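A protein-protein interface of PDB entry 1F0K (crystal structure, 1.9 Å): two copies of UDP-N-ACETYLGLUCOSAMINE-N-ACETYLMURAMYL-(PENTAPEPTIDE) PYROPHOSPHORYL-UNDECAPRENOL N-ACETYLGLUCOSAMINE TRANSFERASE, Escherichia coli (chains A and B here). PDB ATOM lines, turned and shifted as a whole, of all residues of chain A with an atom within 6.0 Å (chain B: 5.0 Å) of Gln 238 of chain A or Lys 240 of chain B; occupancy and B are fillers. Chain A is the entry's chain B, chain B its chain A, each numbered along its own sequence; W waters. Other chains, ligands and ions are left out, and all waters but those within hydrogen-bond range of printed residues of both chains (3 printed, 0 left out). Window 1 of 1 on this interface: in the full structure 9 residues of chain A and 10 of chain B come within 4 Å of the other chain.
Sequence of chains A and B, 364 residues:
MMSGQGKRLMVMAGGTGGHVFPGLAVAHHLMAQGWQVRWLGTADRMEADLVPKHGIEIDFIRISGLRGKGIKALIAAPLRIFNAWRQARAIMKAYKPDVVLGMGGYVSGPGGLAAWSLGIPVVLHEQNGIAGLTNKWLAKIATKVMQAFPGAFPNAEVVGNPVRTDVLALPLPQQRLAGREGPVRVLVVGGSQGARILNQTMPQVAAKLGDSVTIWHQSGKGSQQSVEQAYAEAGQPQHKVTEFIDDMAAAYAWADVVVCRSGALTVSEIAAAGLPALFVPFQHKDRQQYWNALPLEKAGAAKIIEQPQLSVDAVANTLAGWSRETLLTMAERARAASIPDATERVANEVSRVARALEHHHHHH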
ATOM      1  N   GLY A 210       2.531  32.047  23.821  1.00  0.00           N
ATOM      2  CA  GLY A 210       3.697  32.805  23.390  1.00  0.00           C
ATOM      3  C   GLY A 210       4.491  33.511  24.482  1.00  0.00           C
ATOM      4  O   GLY A 210       4.805  32.920  25.517  1.00  0.00           O
ATOM      5  N   ASP A 211       4.796  34.788  24.242  1.00  0.00           N
ATOM      6  CA  ASP A 211       5.579  35.638  25.153  1.00  0.00           C
ATOM      7  C   ASP A 211       5.025  35.880  26.558  1.00  0.00           C
ATOM      8  O   ASP A 211       5.745  36.392  27.426  1.00  0.00           O
ATOM      9  CB  ASP A 211       5.796  37.016  24.517  1.00  0.00           C
ATOM     10  CG  ASP A 211       6.759  36.987  23.356  1.00  0.00           C
ATOM     11  OD1 ASP A 211       6.925  38.043  22.712  1.00  0.00           O
ATOM     12  OD2 ASP A 211       7.356  35.925  23.090  1.00  0.00           O
ATOM     13  N   VAL A 213       4.247  33.758  28.866  1.00  0.00           N
ATOM     14  CA  VAL A 213       4.750  32.851  29.891  1.00  0.00           C
ATOM     15  C   VAL A 213       6.153  32.358  29.569  1.00  0.00           C
ATOM     16  O   VAL A 213       6.593  32.361  28.413  1.00  0.00           O
ATOM     17  CB  VAL A 213       3.870  31.570  30.075  1.00  0.00           C
ATOM     18  CG1 VAL A 213       2.421  31.941  30.372  1.00  0.00           C
ATOM     19  CG2 VAL A 213       3.970  30.680  28.841  1.00  0.00           C
ATOM     20  N   ILE A 215       8.415  29.001  30.672  1.00  0.00           N
ATOM     21  CA  ILE A 215       8.234  27.686  31.255  1.00  0.00           C
ATOM     22  C   ILE A 215       9.500  26.929  31.602  1.00  0.00           C
ATOM     23  O   ILE A 215      10.530  27.068  30.938  1.00  0.00           O
ATOM     24  CB  ILE A 215       7.418  26.794  30.277  1.00  0.00           C
ATOM     25  CG1 ILE A 215       6.041  27.419  30.033  1.00  0.00           C
ATOM     26  CG2 ILE A 215       7.293  25.374  30.822  1.00  0.00           C
ATOM     27  CD1 ILE A 215       5.297  26.849  28.800  1.00  0.00           C
ATOM     28  N   GLU A 228      11.712  18.564  24.744  1.00  0.00           N
ATOM     29  CA  GLU A 228      12.533  19.660  24.232  1.00  0.00           C
ATOM     30  C   GLU A 228      12.212  19.840  22.749  1.00  0.00           C
ATOM     31  O   GLU A 228      12.094  20.963  22.255  1.00  0.00           O
ATOM     32  CB  GLU A 228      14.022  19.332  24.414  1.00  0.00           C
ATOM     33  CG  GLU A 228      14.991  20.374  23.858  1.00  0.00           C
ATOM     34  CD  GLU A 228      15.161  21.589  24.764  1.00  0.00           C
ATOM     35  OE1 GLU A 228      15.781  22.583  24.316  1.00  0.00           O
ATOM     36  OE2 GLU A 228      14.687  21.549  25.920  1.00  0.00           O
ATOM     37  N   GLY A 235       7.367  26.056  18.197  1.00  0.00           N
ATOM     38  CA  GLY A 235       7.894  27.385  17.945  1.00  0.00           C
ATOM     39  C   GLY A 235       8.299  28.176  19.181  1.00  0.00           C
ATOM     40  O   GLY A 235       8.447  29.397  19.112  1.00  0.00           O
ATOM     41  N   GLN A 236       8.469  27.491  20.310  1.00  0.00           N
ATOM     42  CA  GLN A 236       8.872  28.140  21.560  1.00  0.00           C
ATOM     43  C   GLN A 236      10.051  27.358  22.135  1.00  0.00           C
ATOM     44  O   GLN A 236       9.975  26.812  23.235  1.00  0.00           O
ATOM     45  CB  GLN A 236       7.718  28.129  22.569  1.00  0.00           C
ATOM     46  CG  GLN A 236       6.453  28.841  22.127  1.00  0.00           C
ATOM     47  CD  GLN A 236       6.668  30.308  21.822  1.00  0.00           C
ATOM     48  OE1 GLN A 236       7.463  30.984  22.477  1.00  0.00           O
ATOM     49  NE2 GLN A 236       5.943  30.816  20.833  1.00  0.00           N
ATOM     50  N   PRO A 237      11.167  27.307  21.397  1.00  0.00           N
ATOM     51  CA  PRO A 237      12.369  26.583  21.814  1.00  0.00           C
ATOM     52  C   PRO A 237      13.095  27.104  23.052  1.00  0.00           C
ATOM     53  O   PRO A 237      13.860  26.367  23.675  1.00  0.00           O
ATOM     54  CB  PRO A 237      13.251  26.652  20.572  1.00  0.00           C
ATOM     55  CG  PRO A 237      12.936  27.999  20.041  1.00  0.00           C
ATOM     56  CD  PRO A 237      11.421  28.060  20.155  1.00  0.00           C
ATOM     57  N   GLN A 238      12.850  28.361  23.403  1.00  0.00           N
ATOM     58  CA  GLN A 238      13.517  28.978  24.547  1.00  0.00           C
ATOM     59  C   GLN A 238      13.140  28.423  25.918  1.00  0.00           C
ATOM     60  O   GLN A 238      13.862  28.638  26.895  1.00  0.00           O
ATOM     61  CB  GLN A 238      13.284  30.495  24.539  1.00  0.00           C
ATOM     62  CG  GLN A 238      11.892  30.944  24.981  1.00  0.00           C
ATOM     63  CD  GLN A 238      10.817  30.703  23.934  1.00  0.00           C
ATOM     64  OE1 GLN A 238      11.098  30.209  22.839  1.00  0.00           O
ATOM     65  NE2 GLN A 238       9.579  31.057  24.263  1.00  0.00           N
ATOM     66  N   HIS A 239      12.017  27.715  26.012  1.00  0.00           N
ATOM     67  CA  HIS A 239      11.619  27.184  27.309  1.00  0.00           C
ATOM     68  C   HIS A 239      12.599  26.131  27.817  1.00  0.00           C
ATOM     69  O   HIS A 239      13.183  25.374  27.037  1.00  0.00           O
ATOM     70  CB  HIS A 239      10.192  26.630  27.241  1.00  0.00           C
ATOM     71  CG  HIS A 239       9.161  27.681  26.962  1.00  0.00           C
ATOM     72  ND1 HIS A 239       9.067  28.844  27.696  1.00  0.00           N
ATOM     73  CD2 HIS A 239       8.192  27.754  26.017  1.00  0.00           C
ATOM     74  CE1 HIS A 239       8.088  29.589  27.214  1.00  0.00           C
ATOM     75  NE2 HIS A 239       7.542  28.950  26.194  1.00  0.00           N
ATOM     76  N   LYS A 240      12.782  26.102  29.134  1.00  0.00           N
ATOM     77  CA  LYS A 240      13.700  25.171  29.786  1.00  0.00           C
ATOM     78  C   LYS A 240      13.062  23.819  30.060  1.00  0.00           C
ATOM     79  O   LYS A 240      11.985  23.734  30.653  1.00  0.00           O
ATOM     80  CB  LYS A 240      14.180  25.772  31.112  1.00  0.00           C
ATOM     81  CG  LYS A 240      15.185  24.932  31.889  1.00  0.00           C
ATOM     82  CD  LYS A 240      15.317  25.475  33.307  1.00  0.00           C
ATOM     83  CE  LYS A 240      16.387  24.759  34.118  1.00  0.00           C
ATOM     84  NZ  LYS A 240      17.737  25.195  33.698  1.00  0.00           N
ATOM     85  N   VAL A 241      13.739  22.756  29.641  1.00  0.00           N
ATOM     86  CA  VAL A 241      13.242  21.406  29.871  1.00  0.00           C
ATOM     87  C   VAL A 241      14.319  20.564  30.547  1.00  0.00           C
ATOM     88  O   VAL A 241      15.423  20.437  30.029  1.00  0.00           O
ATOM     89  CB  VAL A 241      12.866  20.700  28.557  1.00  0.00           C
ATOM     90  CG1 VAL A 241      12.303  19.315  28.868  1.00  0.00           C
ATOM     91  CG2 VAL A 241      11.870  21.534  27.774  1.00  0.00           C
ATOM     92  N   ILE B 215      18.348  34.069  30.396  1.00  0.00           N
ATOM     93  CA  ILE B 215      19.430  33.548  29.570  1.00  0.00           C
ATOM     94  C   ILE B 215      19.228  32.187  28.914  1.00  0.00           C
ATOM     95  O   ILE B 215      18.589  31.298  29.471  1.00  0.00           O
ATOM     96  CB  ILE B 215      20.725  33.448  30.421  1.00  0.00           C
ATOM     97  CG1 ILE B 215      21.060  34.817  31.020  1.00  0.00           C
ATOM     98  CG2 ILE B 215      21.889  32.943  29.570  1.00  0.00           C
ATOM     99  CD1 ILE B 215      22.212  34.777  32.011  1.00  0.00           C
ATOM    100  N   TRP B 216      19.783  32.054  27.713  1.00  0.00           N
ATOM    101  CA  TRP B 216      19.785  30.794  26.976  1.00  0.00           C
ATOM    102  C   TRP B 216      21.275  30.663  26.696  1.00  0.00           C
ATOM    103  O   TRP B 216      21.807  31.349  25.829  1.00  0.00           O
ATOM    104  CB  TRP B 216      19.034  30.898  25.654  1.00  0.00           C
ATOM    105  CG  TRP B 216      19.059  29.605  24.859  1.00  0.00           C
ATOM    106  CD1 TRP B 216      19.918  28.548  25.017  1.00  0.00           C
ATOM    107  CD2 TRP B 216      18.206  29.266  23.760  1.00  0.00           C
ATOM    108  NE1 TRP B 216      19.649  27.570  24.074  1.00  0.00           N
ATOM    109  CE2 TRP B 216      18.606  27.990  23.292  1.00  0.00           C
ATOM    110  CE3 TRP B 216      17.140  29.915  23.125  1.00  0.00           C
ATOM    111  CZ2 TRP B 216      17.976  27.355  22.215  1.00  0.00           C
ATOM    112  CZ3 TRP B 216      16.511  29.282  22.052  1.00  0.00           C
ATOM    113  CH2 TRP B 216      16.934  28.016  21.609  1.00  0.00           C
ATOM    114  N   HIS B 217      21.937  29.791  27.446  1.00  0.00           N
ATOM    115  CA  HIS B 217      23.381  29.598  27.339  1.00  0.00           C
ATOM    116  C   HIS B 217      23.749  28.308  26.595  1.00  0.00           C
ATOM    117  O   HIS B 217      23.358  27.220  27.006  1.00  0.00           O
ATOM    118  CB  HIS B 217      23.956  29.581  28.765  1.00  0.00           C
ATOM    119  CG  HIS B 217      25.450  29.639  28.835  1.00  0.00           C
ATOM    120  ND1 HIS B 217      26.117  30.491  29.690  1.00  0.00           N
ATOM    121  CD2 HIS B 217      26.406  28.935  28.182  1.00  0.00           C
ATOM    122  CE1 HIS B 217      27.419  30.311  29.561  1.00  0.00           C
ATOM    123  NE2 HIS B 217      27.622  29.372  28.652  1.00  0.00           N
ATOM    124  N   GLN B 238      16.991  28.662  36.797  1.00  0.00           N
ATOM    125  CA  GLN B 238      15.988  28.727  35.735  1.00  0.00           C
ATOM    126  C   GLN B 238      16.495  28.997  34.331  1.00  0.00           C
ATOM    127  O   GLN B 238      15.776  28.755  33.358  1.00  0.00           O
ATOM    128  CB  GLN B 238      14.917  29.776  36.063  1.00  0.00           C
ATOM    129  CG  GLN B 238      15.354  31.230  35.925  1.00  0.00           C
ATOM    130  CD  GLN B 238      16.238  31.694  37.068  1.00  0.00           C
ATOM    131  OE1 GLN B 238      16.375  31.008  38.077  1.00  0.00           O
ATOM    132  NE2 GLN B 238      16.830  32.870  36.915  1.00  0.00           N
ATOM    133  N   HIS B 239      17.713  29.505  34.205  1.00  0.00           N
ATOM    134  CA  HIS B 239      18.229  29.797  32.879  1.00  0.00           C
ATOM    135  C   HIS B 239      18.388  28.529  32.053  1.00  0.00           C
ATOM    136  O   HIS B 239      18.699  27.464  32.588  1.00  0.00           O
ATOM    137  CB  HIS B 239      19.551  30.559  32.982  1.00  0.00           C
ATOM    138  CG  HIS B 239      19.402  31.923  33.581  1.00  0.00           C
ATOM    139  ND1 HIS B 239      18.449  32.820  33.151  1.00  0.00           N
ATOM    140  CD2 HIS B 239      20.080  32.543  34.578  1.00  0.00           C
ATOM    141  CE1 HIS B 239      18.546  33.935  33.854  1.00  0.00           C
ATOM    142  NE2 HIS B 239      19.527  33.792  34.727  1.00  0.00           N
ATOM    143  N   LYS B 240      18.152  28.655  30.748  1.00  0.00           N
ATOM    144  CA  LYS B 240      18.255  27.523  29.824  1.00  0.00           C
ATOM    145  C   LYS B 240      19.697  27.284  29.405  1.00  0.00           C
ATOM    146  O   LYS B 240      20.380  28.210  28.979  1.00  0.00           O
ATOM    147  CB  LYS B 240      17.413  27.796  28.572  1.00  0.00           C
ATOM    148  CG  LYS B 240      17.362  26.659  27.531  1.00  0.00           C
ATOM    149  CD  LYS B 240      16.623  27.133  26.280  1.00  0.00           C
ATOM    150  CE  LYS B 240      16.475  26.046  25.203  1.00  0.00           C
ATOM    151  NZ  LYS B 240      15.489  24.979  25.572  1.00  0.00           N
ATOM    152  N   VAL B 241      20.149  26.039  29.510  1.00  0.00           N
ATOM    153  CA  VAL B 241      21.505  25.675  29.109  1.00  0.00           C
ATOM    154  C   VAL B 241      21.455  24.473  28.167  1.00  0.00           C
ATOM    155  O   VAL B 241      20.917  23.426  28.521  1.00  0.00           O
ATOM    156  CB  VAL B 241      22.386  25.287  30.314  1.00  0.00           C
ATOM    157  CG1 VAL B 241      23.809  24.989  29.839  1.00  0.00           C
ATOM    158  CG2 VAL B 241      22.396  26.415  31.336  1.00  0.00           C
ATOM    159  N   THR B 242      21.999  24.634  26.968  1.00  0.00           N
ATOM    160  CA  THR B 242      22.018  23.542  26.000  1.00  0.00           C
ATOM    161  C   THR B 242      23.435  23.328  25.488  1.00  0.00           C
ATOM    162  O   THR B 242      24.220  24.273  25.358  1.00  0.00           O
ATOM    163  CB  THR B 242      21.080  23.812  24.794  1.00  0.00           C
ATOM    164  OG1 THR B 242      21.428  25.055  24.174  1.00  0.00           O
ATOM    165  CG2 THR B 242      19.628  23.864  25.246  1.00  0.00           C
ATOM    166  N   TRP B 254      14.309  34.792  19.065  1.00  0.00           N
ATOM    167  CA  TRP B 254      13.982  34.967  20.479  1.00  0.00           C
ATOM    168  C   TRP B 254      14.792  36.037  21.212  1.00  0.00           C
ATOM    169  O   TRP B 254      14.235  36.833  21.970  1.00  0.00           O
ATOM    170  CB  TRP B 254      14.173  33.637  21.204  1.00  0.00           C
ATOM    171  CG  TRP B 254      14.162  33.747  22.698  1.00  0.00           C
ATOM    172  CD1 TRP B 254      13.067  33.777  23.510  1.00  0.00           C
ATOM    173  CD2 TRP B 254      15.306  33.837  23.559  1.00  0.00           C
ATOM    174  NE1 TRP B 254      13.458  33.872  24.828  1.00  0.00           N
ATOM    175  CE2 TRP B 254      14.826  33.912  24.886  1.00  0.00           C
ATOM    176  CE3 TRP B 254      16.690  33.863  23.338  1.00  0.00           C
ATOM    177  CZ2 TRP B 254      15.686  34.011  25.996  1.00  0.00           C
ATOM    178  CZ3 TRP B 254      17.548  33.964  24.442  1.00  0.00           C
ATOM    179  CH2 TRP B 254      17.037  34.036  25.754  1.00  0.00           C
HETATM  180  O   HOH W   1      18.815  24.221  31.177  1.00  0.00           O
HETATM  181  O   HOH W   2      20.581  26.528  34.433  1.00  0.00           O
HETATM  182  O   HOH W   3      16.001  23.224  27.659  1.00  0.00           O
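Of the 12 printed residues of chain A, 5 touch a printed residue of chain B. Hydrophobic or aromatic side chains of chain B within 4 Å of the printed part of chain A: Trp 216 and Trp 254. Among the printed residues, 8 pairs touch across the chains. Among the printed residues, Asp or Glu carboxylates within 4 Å of a Lys or Arg side-chain nitrogen of the other chain: Glu 228 of chain A with Lys 240 of chain B.
Water W3 lies within hydrogen-bond range of the side-chain carboxylate of Glu 228 of chain A (2.7 Å), the side-chain amino group of Lys 240 of chain B (2.8 Å) and the backbone NH of Val 241 of chain A (3.0 Å). Water W2 lies within hydrogen-bond range of O of His 239 of chain B (2.8 Å) and NZ of Lys 240 of chain A (3.2 Å). Water W1 bridges N of Val 241 of chain B (2.8 Å) and NZ of Lys 240 of chain A (2.9 Å).
Asp 211 of chain A touches none of the printed residues of chain B. Printed residues of chain B within 4 Å of Glu 228 of chain A: Lys 240 (2.7 Å). Gln 238 of chain A touches just these residues of chain B: Trp 216 (3.9 Å), Lys 240 (3.2 Å) and Trp 254 (3.3 Å). Printed residues of chain A within 4 Å of Trp 216 of chain B: Gln 238 (3.9 Å). Lys 240 of chain B touches just these residues of chain A: Glu 228 (2.7 Å), Pro 237 (2.9 Å), Gln 238 (3.2 Å) and His 239 (2.8 Å). The nearest printed residue of chain B that does not touch Gln 238 of chain A is Ile 215 of chain B (6.0 Å). The nearest residue of chain A that does not touch Lys 240 of chain B is Lys 240 of chain A (4.5 Å).
Gln 238 of chain A touches Trp 216 of chain B (CA to CZ3, 3.9 Å). Gln 238 of chain A touches Lys 240 of chain B. Gln 238 of chain A touches Trp 254 of chain B (CG to NE1, 3.3 Å). O of Gln 238 of chain B touches CD of Lys 240 of chain A (3.3 Å).
The side-chain carboxylate (OE1) of Glu 228 of chain A is in salt-bridge range of the side-chain amino group (NZ) of Lys 240 of chain B (2.7 Å). The side-chain amino group (NZ) of Lys 240 of chain A lies within hydrogen-bond range of the backbone carbonyl oxygen (O) of His 239 of chain B, 2.7 Å away. O of His 239 of chain A sits at hydrogen-bond distance from NZ of Lys 240 of chain B (2.8 Å). NZ of Lys 240 of chain B sits at hydrogen-bond distance from O of Pro 237 of chain A, at 2.9 Å.
ND1 of His 239 of chain B lies within hydrogen-bond range of N of Ile 215 of chain B. OG1 of Thr 242 of chain B sits at hydrogen-bond distance from NE1 of Trp 216 of chain B, 3.1 Å away. N of Lys 240 of chain B sits at hydrogen-bond distance from O of Ile 215 of chain B, at 3.0 Å. The side-chain amide nitrogen (NE2) of Gln 238 of chain A sits at hydrogen-bond distance from the side-chain amide oxygen (OE1) of Gln 236 of chain A (2.8 Å). The backbone carbonyl oxygen of Ile 215 of chain A is in hydrogen-bond range of the backbone NH of Lys 240 of chain A (3.0 Å). ND1 of His 239 of chain A sits at hydrogen-bond distance from N of Ile 215 of chain A (3.1 Å).
Gln 238 of chain A touches Lys 240 of chain B, and with the chains exchanged Lys 240 of chain A touches Gln 238 of chain B. His 239 of chain A touches Lys 240 of chain B, and with the chains exchanged Lys 240 of chain A touches His 239 of chain B. Of the 8 pairs that touch across the chains among the printed residues, 4 have their exchanged pair printed and touching as well.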
